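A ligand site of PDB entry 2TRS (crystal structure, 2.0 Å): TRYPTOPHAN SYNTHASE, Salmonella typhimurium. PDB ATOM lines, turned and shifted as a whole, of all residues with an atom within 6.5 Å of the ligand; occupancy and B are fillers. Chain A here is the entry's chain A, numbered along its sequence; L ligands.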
ATOM      1  N   PHE A  22     -16.788  -8.730 -20.587  1.00  0.00           N
ATOM      2  CA  PHE A  22     -18.220  -8.620 -20.752  1.00  0.00           C
ATOM      3  C   PHE A  22     -18.420  -7.871 -22.083  1.00  0.00           C
ATOM      4  O   PHE A  22     -17.707  -6.880 -22.284  1.00  0.00           O
ATOM      5  CB  PHE A  22     -18.783  -7.858 -19.541  1.00  0.00           C
ATOM      6  CG  PHE A  22     -20.207  -7.432 -19.822  1.00  0.00           C
ATOM      7  CD1 PHE A  22     -20.469  -6.177 -20.415  1.00  0.00           C
ATOM      8  CD2 PHE A  22     -21.239  -8.342 -19.601  1.00  0.00           C
ATOM      9  CE1 PHE A  22     -21.771  -5.856 -20.787  1.00  0.00           C
ATOM     10  CE2 PHE A  22     -22.531  -8.011 -19.977  1.00  0.00           C
ATOM     11  CZ  PHE A  22     -22.796  -6.778 -20.577  1.00  0.00           C
ATOM     12  N   GLU A  49     -18.895 -13.224 -20.667  1.00  0.00           N
ATOM     13  CA  GLU A  49     -20.137 -12.757 -20.055  1.00  0.00           C
ATOM     14  C   GLU A  49     -20.787 -11.952 -21.175  1.00  0.00           C
ATOM     15  O   GLU A  49     -20.194 -10.989 -21.666  1.00  0.00           O
ATOM     16  CB  GLU A  49     -19.880 -11.853 -18.874  1.00  0.00           C
ATOM     17  CG  GLU A  49     -21.105 -11.741 -17.971  1.00  0.00           C
ATOM     18  CD  GLU A  49     -21.442 -13.025 -17.249  1.00  0.00           C
ATOM     19  OE1 GLU A  49     -22.619 -13.346 -17.058  1.00  0.00           O
ATOM     20  OE2 GLU A  49     -20.505 -13.725 -16.892  1.00  0.00           O
ATOM     21  N   ALA A  59     -29.586  -1.492 -14.241  1.00  0.00           N
ATOM     22  CA  ALA A  59     -28.317  -1.622 -13.527  1.00  0.00           C
ATOM     23  C   ALA A  59     -27.078  -1.256 -14.335  1.00  0.00           C
ATOM     24  O   ALA A  59     -25.915  -1.377 -13.939  1.00  0.00           O
ATOM     25  CB  ALA A  59     -28.176  -3.060 -13.054  1.00  0.00           C
ATOM     26  N   ASP A  60     -27.338  -0.640 -15.476  1.00  0.00           N
ATOM     27  CA  ASP A  60     -26.291  -0.301 -16.375  1.00  0.00           C
ATOM     28  C   ASP A  60     -26.201   1.166 -16.635  1.00  0.00           C
ATOM     29  O   ASP A  60     -27.108   1.791 -17.166  1.00  0.00           O
ATOM     30  CB  ASP A  60     -26.479  -1.024 -17.666  1.00  0.00           C
ATOM     31  CG  ASP A  60     -25.941  -2.437 -17.595  1.00  0.00           C
ATOM     32  OD1 ASP A  60     -24.733  -2.547 -17.631  1.00  0.00           O
ATOM     33  OD2 ASP A  60     -26.706  -3.397 -17.515  1.00  0.00           O
ATOM     34  N   ILE A  64     -22.611   0.975 -21.374  1.00  0.00           N
ATOM     35  CA  ILE A  64     -23.386  -0.200 -21.683  1.00  0.00           C
ATOM     36  C   ILE A  64     -24.722   0.257 -22.205  1.00  0.00           C
ATOM     37  O   ILE A  64     -25.253  -0.371 -23.119  1.00  0.00           O
ATOM     38  CB  ILE A  64     -23.533  -1.072 -20.424  1.00  0.00           C
ATOM     39  CG1 ILE A  64     -22.119  -1.576 -20.038  1.00  0.00           C
ATOM     40  CG2 ILE A  64     -24.503  -2.216 -20.687  1.00  0.00           C
ATOM     41  CD1 ILE A  64     -21.810  -2.457 -18.826  1.00  0.00           C
ATOM     42  N   LEU A 100     -25.930 -12.160 -19.440  1.00  0.00           N
ATOM     43  CA  LEU A 100     -26.374 -11.168 -18.473  1.00  0.00           C
ATOM     44  C   LEU A 100     -27.758 -10.705 -18.962  1.00  0.00           C
ATOM     45  O   LEU A 100     -27.858 -10.050 -20.004  1.00  0.00           O
ATOM     46  CB  LEU A 100     -25.414  -9.977 -18.409  1.00  0.00           C
ATOM     47  CG  LEU A 100     -25.606  -9.071 -17.177  1.00  0.00           C
ATOM     48  CD1 LEU A 100     -26.614  -7.968 -17.491  1.00  0.00           C
ATOM     49  CD2 LEU A 100     -26.085  -9.900 -15.990  1.00  0.00           C
ATOM     50  N   TYR A 102     -32.045  -9.262 -18.231  1.00  0.00           N
ATOM     51  CA  TYR A 102     -33.035  -8.504 -17.494  1.00  0.00           C
ATOM     52  C   TYR A 102     -34.271  -9.340 -17.584  1.00  0.00           C
ATOM     53  O   TYR A 102     -34.544  -9.917 -18.638  1.00  0.00           O
ATOM     54  CB  TYR A 102     -33.235  -7.167 -18.144  1.00  0.00           C
ATOM     55  CG  TYR A 102     -32.187  -6.204 -17.620  1.00  0.00           C
ATOM     56  CD1 TYR A 102     -32.288  -5.723 -16.317  1.00  0.00           C
ATOM     57  CD2 TYR A 102     -31.143  -5.819 -18.446  1.00  0.00           C
ATOM     58  CE1 TYR A 102     -31.322  -4.849 -15.810  1.00  0.00           C
ATOM     59  CE2 TYR A 102     -30.176  -4.950 -17.953  1.00  0.00           C
ATOM     60  CZ  TYR A 102     -30.269  -4.475 -16.646  1.00  0.00           C
ATOM     61  OH  TYR A 102     -29.243  -3.681 -16.152  1.00  0.00           O
ATOM     62  N   LEU A 127     -27.426 -14.821 -15.589  1.00  0.00           N
ATOM     63  CA  LEU A 127     -27.551 -13.932 -14.431  1.00  0.00           C
ATOM     64  C   LEU A 127     -28.722 -13.031 -14.761  1.00  0.00           C
ATOM     65  O   LEU A 127     -28.685 -12.324 -15.800  1.00  0.00           O
ATOM     66  CB  LEU A 127     -26.314 -13.013 -14.266  1.00  0.00           C
ATOM     67  CG  LEU A 127     -25.819 -12.441 -12.940  1.00  0.00           C
ATOM     68  CD1 LEU A 127     -24.694 -11.448 -13.224  1.00  0.00           C
ATOM     69  CD2 LEU A 127     -26.941 -11.753 -12.185  1.00  0.00           C
ATOM     70  N   ALA A 129     -30.233  -9.836 -13.757  1.00  0.00           N
ATOM     71  CA  ALA A 129     -29.784  -8.638 -13.059  1.00  0.00           C
ATOM     72  C   ALA A 129     -30.804  -8.059 -12.091  1.00  0.00           C
ATOM     73  O   ALA A 129     -30.433  -7.622 -10.994  1.00  0.00           O
ATOM     74  CB  ALA A 129     -29.381  -7.583 -14.115  1.00  0.00           C
ATOM     75  N   ILE A 153     -26.031 -12.360  -7.432  1.00  0.00           N
ATOM     76  CA  ILE A 153     -25.103 -11.320  -6.996  1.00  0.00           C
ATOM     77  C   ILE A 153     -25.078 -11.295  -5.486  1.00  0.00           C
ATOM     78  O   ILE A 153     -26.085 -11.522  -4.808  1.00  0.00           O
ATOM     79  CB  ILE A 153     -25.542  -9.935  -7.549  1.00  0.00           C
ATOM     80  CG1 ILE A 153     -25.509 -10.036  -9.058  1.00  0.00           C
ATOM     81  CG2 ILE A 153     -24.633  -8.803  -7.035  1.00  0.00           C
ATOM     82  CD1 ILE A 153     -25.705  -8.734  -9.839  1.00  0.00           C
ATOM     83  N   TYR A 175     -21.354 -13.875  -8.357  1.00  0.00           N
ATOM     84  CA  TYR A 175     -20.935 -12.559  -8.822  1.00  0.00           C
ATOM     85  C   TYR A 175     -20.781 -11.787  -7.514  1.00  0.00           C
ATOM     86  O   TYR A 175     -21.743 -11.676  -6.740  1.00  0.00           O
ATOM     87  CB  TYR A 175     -21.999 -11.941  -9.722  1.00  0.00           C
ATOM     88  CG  TYR A 175     -21.588 -10.669 -10.450  1.00  0.00           C
ATOM     89  CD1 TYR A 175     -21.616  -9.410  -9.824  1.00  0.00           C
ATOM     90  CD2 TYR A 175     -21.183 -10.743 -11.767  1.00  0.00           C
ATOM     91  CE1 TYR A 175     -21.229  -8.245 -10.514  1.00  0.00           C
ATOM     92  CE2 TYR A 175     -20.804  -9.593 -12.468  1.00  0.00           C
ATOM     93  CZ  TYR A 175     -20.827  -8.357 -11.833  1.00  0.00           C
ATOM     94  OH  TYR A 175     -20.434  -7.240 -12.535  1.00  0.00           O
ATOM     95  N   LEU A 177     -20.028  -8.295  -5.725  1.00  0.00           N
ATOM     96  CA  LEU A 177     -20.067  -6.903  -6.100  1.00  0.00           C
ATOM     97  C   LEU A 177     -19.069  -6.084  -5.322  1.00  0.00           C
ATOM     98  O   LEU A 177     -19.159  -5.947  -4.094  1.00  0.00           O
ATOM     99  CB  LEU A 177     -21.433  -6.271  -5.843  1.00  0.00           C
ATOM    100  CG  LEU A 177     -22.343  -5.810  -6.963  1.00  0.00           C
ATOM    101  CD1 LEU A 177     -23.441  -5.049  -6.256  1.00  0.00           C
ATOM    102  CD2 LEU A 177     -21.660  -4.951  -8.014  1.00  0.00           C
ATOM    103  N   ARG A 179     -18.509  -2.658  -5.233  1.00  0.00           N
ATOM    104  CA  ARG A 179     -18.966  -1.251  -5.206  1.00  0.00           C
ATOM    105  C   ARG A 179     -20.486  -1.223  -5.134  1.00  0.00           C
ATOM    106  O   ARG A 179     -21.100  -2.203  -4.698  1.00  0.00           O
ATOM    107  CB  ARG A 179     -18.564  -0.402  -6.436  1.00  0.00           C
ATOM    108  CG  ARG A 179     -19.162  -0.604  -7.821  1.00  0.00           C
ATOM    109  CD  ARG A 179     -18.877   0.771  -8.413  1.00  0.00           C
ATOM    110  NE  ARG A 179     -18.820   0.835  -9.869  1.00  0.00           N
ATOM    111  CZ  ARG A 179     -19.850   1.184 -10.659  1.00  0.00           C
ATOM    112  NH1 ARG A 179     -21.040   1.515 -10.130  1.00  0.00           N
ATOM    113  NH2 ARG A 179     -19.648   1.250 -11.987  1.00  0.00           N
ATOM    114  N   VAL A 182     -24.339   1.573 -10.756  1.00  0.00           N
ATOM    115  CA  VAL A 182     -24.627   1.030 -12.065  1.00  0.00           C
ATOM    116  C   VAL A 182     -23.305   1.031 -12.824  1.00  0.00           C
ATOM    117  O   VAL A 182     -22.431   1.868 -12.557  1.00  0.00           O
ATOM    118  CB  VAL A 182     -25.703   1.906 -12.819  1.00  0.00           C
ATOM    119  CG1 VAL A 182     -27.041   1.622 -12.145  1.00  0.00           C
ATOM    120  CG2 VAL A 182     -25.413   3.417 -12.782  1.00  0.00           C
ATOM    121  N   THR A 183     -23.160   0.105 -13.786  1.00  0.00           N
ATOM    122  CA  THR A 183     -21.916  -0.121 -14.518  1.00  0.00           C
ATOM    123  C   THR A 183     -21.139   1.089 -15.097  1.00  0.00           C
ATOM    124  O   THR A 183     -21.721   1.968 -15.750  1.00  0.00           O
ATOM    125  CB  THR A 183     -22.239  -1.119 -15.660  1.00  0.00           C
ATOM    126  OG1 THR A 183     -23.205  -0.510 -16.513  1.00  0.00           O
ATOM    127  CG2 THR A 183     -22.850  -2.399 -15.181  1.00  0.00           C
ATOM    128  N   GLY A 184     -19.811   1.156 -14.944  1.00  0.00           N
ATOM    129  CA  GLY A 184     -19.041   2.235 -15.543  1.00  0.00           C
ATOM    130  C   GLY A 184     -17.551   2.010 -15.317  1.00  0.00           C
ATOM    131  O   GLY A 184     -17.148   1.217 -14.457  1.00  0.00           O
ATOM    132  N   ALA A 185     -16.720   2.626 -16.180  1.00  0.00           N
ATOM    133  CA  ALA A 185     -15.257   2.531 -16.065  1.00  0.00           C
ATOM    134  C   ALA A 185     -14.696   3.718 -15.288  1.00  0.00           C
ATOM    135  O   ALA A 185     -13.648   4.312 -15.572  1.00  0.00           O
ATOM    136  CB  ALA A 185     -14.628   2.507 -17.471  1.00  0.00           C
ATOM    137  N   GLY A 211     -16.898  -8.155  -9.260  1.00  0.00           N
ATOM    138  CA  GLY A 211     -17.928  -7.337  -9.869  1.00  0.00           C
ATOM    139  C   GLY A 211     -17.650  -6.090 -10.664  1.00  0.00           C
ATOM    140  O   GLY A 211     -16.850  -6.027 -11.595  1.00  0.00           O
ATOM    141  N   PHE A 212     -18.482  -5.086 -10.349  1.00  0.00           N
ATOM    142  CA  PHE A 212     -18.344  -3.810 -11.027  1.00  0.00           C
ATOM    143  C   PHE A 212     -17.114  -3.194 -10.387  1.00  0.00           C
ATOM    144  O   PHE A 212     -16.792  -3.534  -9.231  1.00  0.00           O
ATOM    145  CB  PHE A 212     -19.438  -2.752 -10.762  1.00  0.00           C
ATOM    146  CG  PHE A 212     -20.881  -2.915 -11.189  1.00  0.00           C
ATOM    147  CD1 PHE A 212     -21.305  -3.886 -12.105  1.00  0.00           C
ATOM    148  CD2 PHE A 212     -21.821  -2.034 -10.638  1.00  0.00           C
ATOM    149  CE1 PHE A 212     -22.642  -3.982 -12.445  1.00  0.00           C
ATOM    150  CE2 PHE A 212     -23.162  -2.142 -10.997  1.00  0.00           C
ATOM    151  CZ  PHE A 212     -23.587  -3.108 -11.900  1.00  0.00           C
ATOM    152  N   GLY A 213     -16.467  -2.293 -11.132  1.00  0.00           N
ATOM    153  CA  GLY A 213     -15.341  -1.572 -10.597  1.00  0.00           C
ATOM    154  C   GLY A 213     -14.079  -2.421 -10.583  1.00  0.00           C
ATOM    155  O   GLY A 213     -13.487  -2.707  -9.523  1.00  0.00           O
ATOM    156  N   ILE A 214     -13.704  -2.898 -11.775  1.00  0.00           N
ATOM    157  CA  ILE A 214     -12.432  -3.584 -12.009  1.00  0.00           C
ATOM    158  C   ILE A 214     -11.979  -2.799 -13.227  1.00  0.00           C
ATOM    159  O   ILE A 214     -12.718  -2.532 -14.190  1.00  0.00           O
ATOM    160  CB  ILE A 214     -12.564  -5.094 -12.363  1.00  0.00           C
ATOM    161  CG1 ILE A 214     -13.095  -5.905 -11.177  1.00  0.00           C
ATOM    162  CG2 ILE A 214     -11.200  -5.634 -12.775  1.00  0.00           C
ATOM    163  CD1 ILE A 214     -12.315  -5.916  -9.854  1.00  0.00           C
ATOM    164  N   ILE A 232     -14.272  -9.754 -13.658  1.00  0.00           N
ATOM    165  CA  ILE A 232     -15.044  -9.448 -14.848  1.00  0.00           C
ATOM    166  C   ILE A 232     -14.880  -7.980 -15.195  1.00  0.00           C
ATOM    167  O   ILE A 232     -14.847  -7.118 -14.312  1.00  0.00           O
ATOM    168  CB  ILE A 232     -16.586  -9.777 -14.645  1.00  0.00           C
ATOM    169  CG1 ILE A 232     -16.751 -11.223 -14.170  1.00  0.00           C
ATOM    170  CG2 ILE A 232     -17.371  -9.556 -15.956  1.00  0.00           C
ATOM    171  CD1 ILE A 232     -18.171 -11.683 -13.821  1.00  0.00           C
ATOM    172  N   SER A 233     -14.787  -7.657 -16.488  1.00  0.00           N
ATOM    173  CA  SER A 233     -14.632  -6.297 -16.946  1.00  0.00           C
ATOM    174  C   SER A 233     -15.492  -6.104 -18.190  1.00  0.00           C
ATOM    175  O   SER A 233     -15.557  -6.977 -19.048  1.00  0.00           O
ATOM    176  CB  SER A 233     -13.140  -6.095 -17.196  1.00  0.00           C
ATOM    177  OG  SER A 233     -12.797  -4.814 -17.720  1.00  0.00           O
ATOM    178  N   GLY A 234     -16.168  -4.961 -18.357  1.00  0.00           N
ATOM    179  CA  GLY A 234     -17.044  -4.735 -19.516  1.00  0.00           C
ATOM    180  C   GLY A 234     -16.850  -3.315 -20.017  1.00  0.00           C
ATOM    181  O   GLY A 234     -16.510  -3.051 -21.161  1.00  0.00           O
ATOM    182  N   SER A 235     -17.010  -2.406 -19.057  1.00  0.00           N
ATOM    183  CA  SER A 235     -16.766  -0.972 -19.145  1.00  0.00           C
ATOM    184  C   SER A 235     -15.661  -0.557 -20.107  1.00  0.00           C
ATOM    185  O   SER A 235     -15.877   0.093 -21.137  1.00  0.00           O
ATOM    186  CB  SER A 235     -16.434  -0.505 -17.759  1.00  0.00           C
ATOM    187  OG  SER A 235     -15.593  -1.481 -17.109  1.00  0.00           O
ATOM    188  N   ALA A 236     -14.482  -1.039 -19.727  1.00  0.00           N
ATOM    189  CA  ALA A 236     -13.236  -0.823 -20.418  1.00  0.00           C
ATOM    190  C   ALA A 236     -13.334  -1.280 -21.863  1.00  0.00           C
ATOM    191  O   ALA A 236     -13.211  -0.470 -22.791  1.00  0.00           O
ATOM    192  CB  ALA A 236     -12.165  -1.596 -19.672  1.00  0.00           C
HETATM  193  N1  LIG L   1     -24.067  -5.104 -16.676  1.00  0.00           N
HETATM  194  C1  LIG L   1     -22.800  -5.692 -16.932  1.00  0.00           C
HETATM  195  C2  LIG L   1     -22.489  -6.444 -15.873  1.00  0.00           C
HETATM  196  C3  LIG L   1     -23.842  -6.910 -13.645  1.00  0.00           C
HETATM  197  C4  LIG L   1     -25.096  -6.545 -13.011  1.00  0.00           C
HETATM  198  C5  LIG L   1     -25.989  -5.676 -13.617  1.00  0.00           C
HETATM  199  C6  LIG L   1     -25.712  -5.120 -14.880  1.00  0.00           C
HETATM  200  C7  LIG L   1     -24.507  -5.475 -15.506  1.00  0.00           C
HETATM  201  C8  LIG L   1     -23.567  -6.350 -14.933  1.00  0.00           C
HETATM  202  C9  LIG L   1     -19.717  -5.097 -14.741  1.00  0.00           C
HETATM  203  C10 LIG L   1     -20.024  -6.377 -15.461  1.00  0.00           C
HETATM  204  C11 LIG L   1     -21.216  -7.269 -15.724  1.00  0.00           C
HETATM  205  P1  LIG L   1     -18.336  -2.941 -15.359  1.00  0.00           P
HETATM  206  O1  LIG L   1     -18.743  -2.029 -16.452  1.00  0.00           O
HETATM  207  O2  LIG L   1     -16.936  -3.622 -15.634  1.00  0.00           O
HETATM  208  O3  LIG L   1     -18.242  -2.341 -13.983  1.00  0.00           O
HETATM  209  O4  LIG L   1     -19.391  -4.050 -15.421  1.00  0.00           O
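The backbone NH (N) of Gly 213 sits at hydrogen-bond distance from an oxygen (O3) of the ligand (3.4 Å). N of Ser 235 lies close to O1 of the ligand (3.2 Å). O2 of the ligand lies within hydrogen-bond range of N of Gly 234, 3.1 Å away. The side-chain carboxylate (OD1) of Asp 60 is in hydrogen-bond range of a nitrogen (N1) of the ligand, at 2.8 Å. An oxygen (O2) of the ligand is in hydrogen-bond range of the side-chain hydroxyl of Ser 235, at 2.9 Å.
The backbone carbonyl oxygen (O) of Ser 233 sits at hydrogen-bond distance from the backbone NH (N) of Phe 22. The side-chain hydroxyl (OH) of Tyr 102 lies within hydrogen-bond range of the backbone NH (N) of Ala 59 (2.9 Å). N of Thr 183 sits at hydrogen-bond distance from O of Ala 59 (3.1 Å). OD2 of Asp 60 is in hydrogen-bond range of OH of Tyr 102 (2.9 Å). The side-chain carboxylate (OD1) of Asp 60 sits at hydrogen-bond distance from the side-chain hydroxyl (OG1) of Thr 183 (2.8 Å).
Phe 22 touches the ligand. Ala 59 touches the ligand. Ile 64 touches the ligand. Leu 100 touches the ligand (CD1 to C7, 3.8 Å). Ala 129 touches the ligand (CB to C5, 3.9 Å). Ile 153 touches the ligand (CD1 to C4, 3.9 Å). Tyr 175 touches the ligand. Thr 183 touches the ligand. Gly 184 touches the ligand. Phe 212 touches the ligand. CA of Ser 233 touches O2 of the ligand, 3.8 Å away. Of the 26 residues printed, 15 come within 4 Å of the ligand. Along chain A the residues within 4 Å of the ligand span positions 22 to 235. The nearest printed residue that does not touch the ligand is Tyr 102 (4.02 Å).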
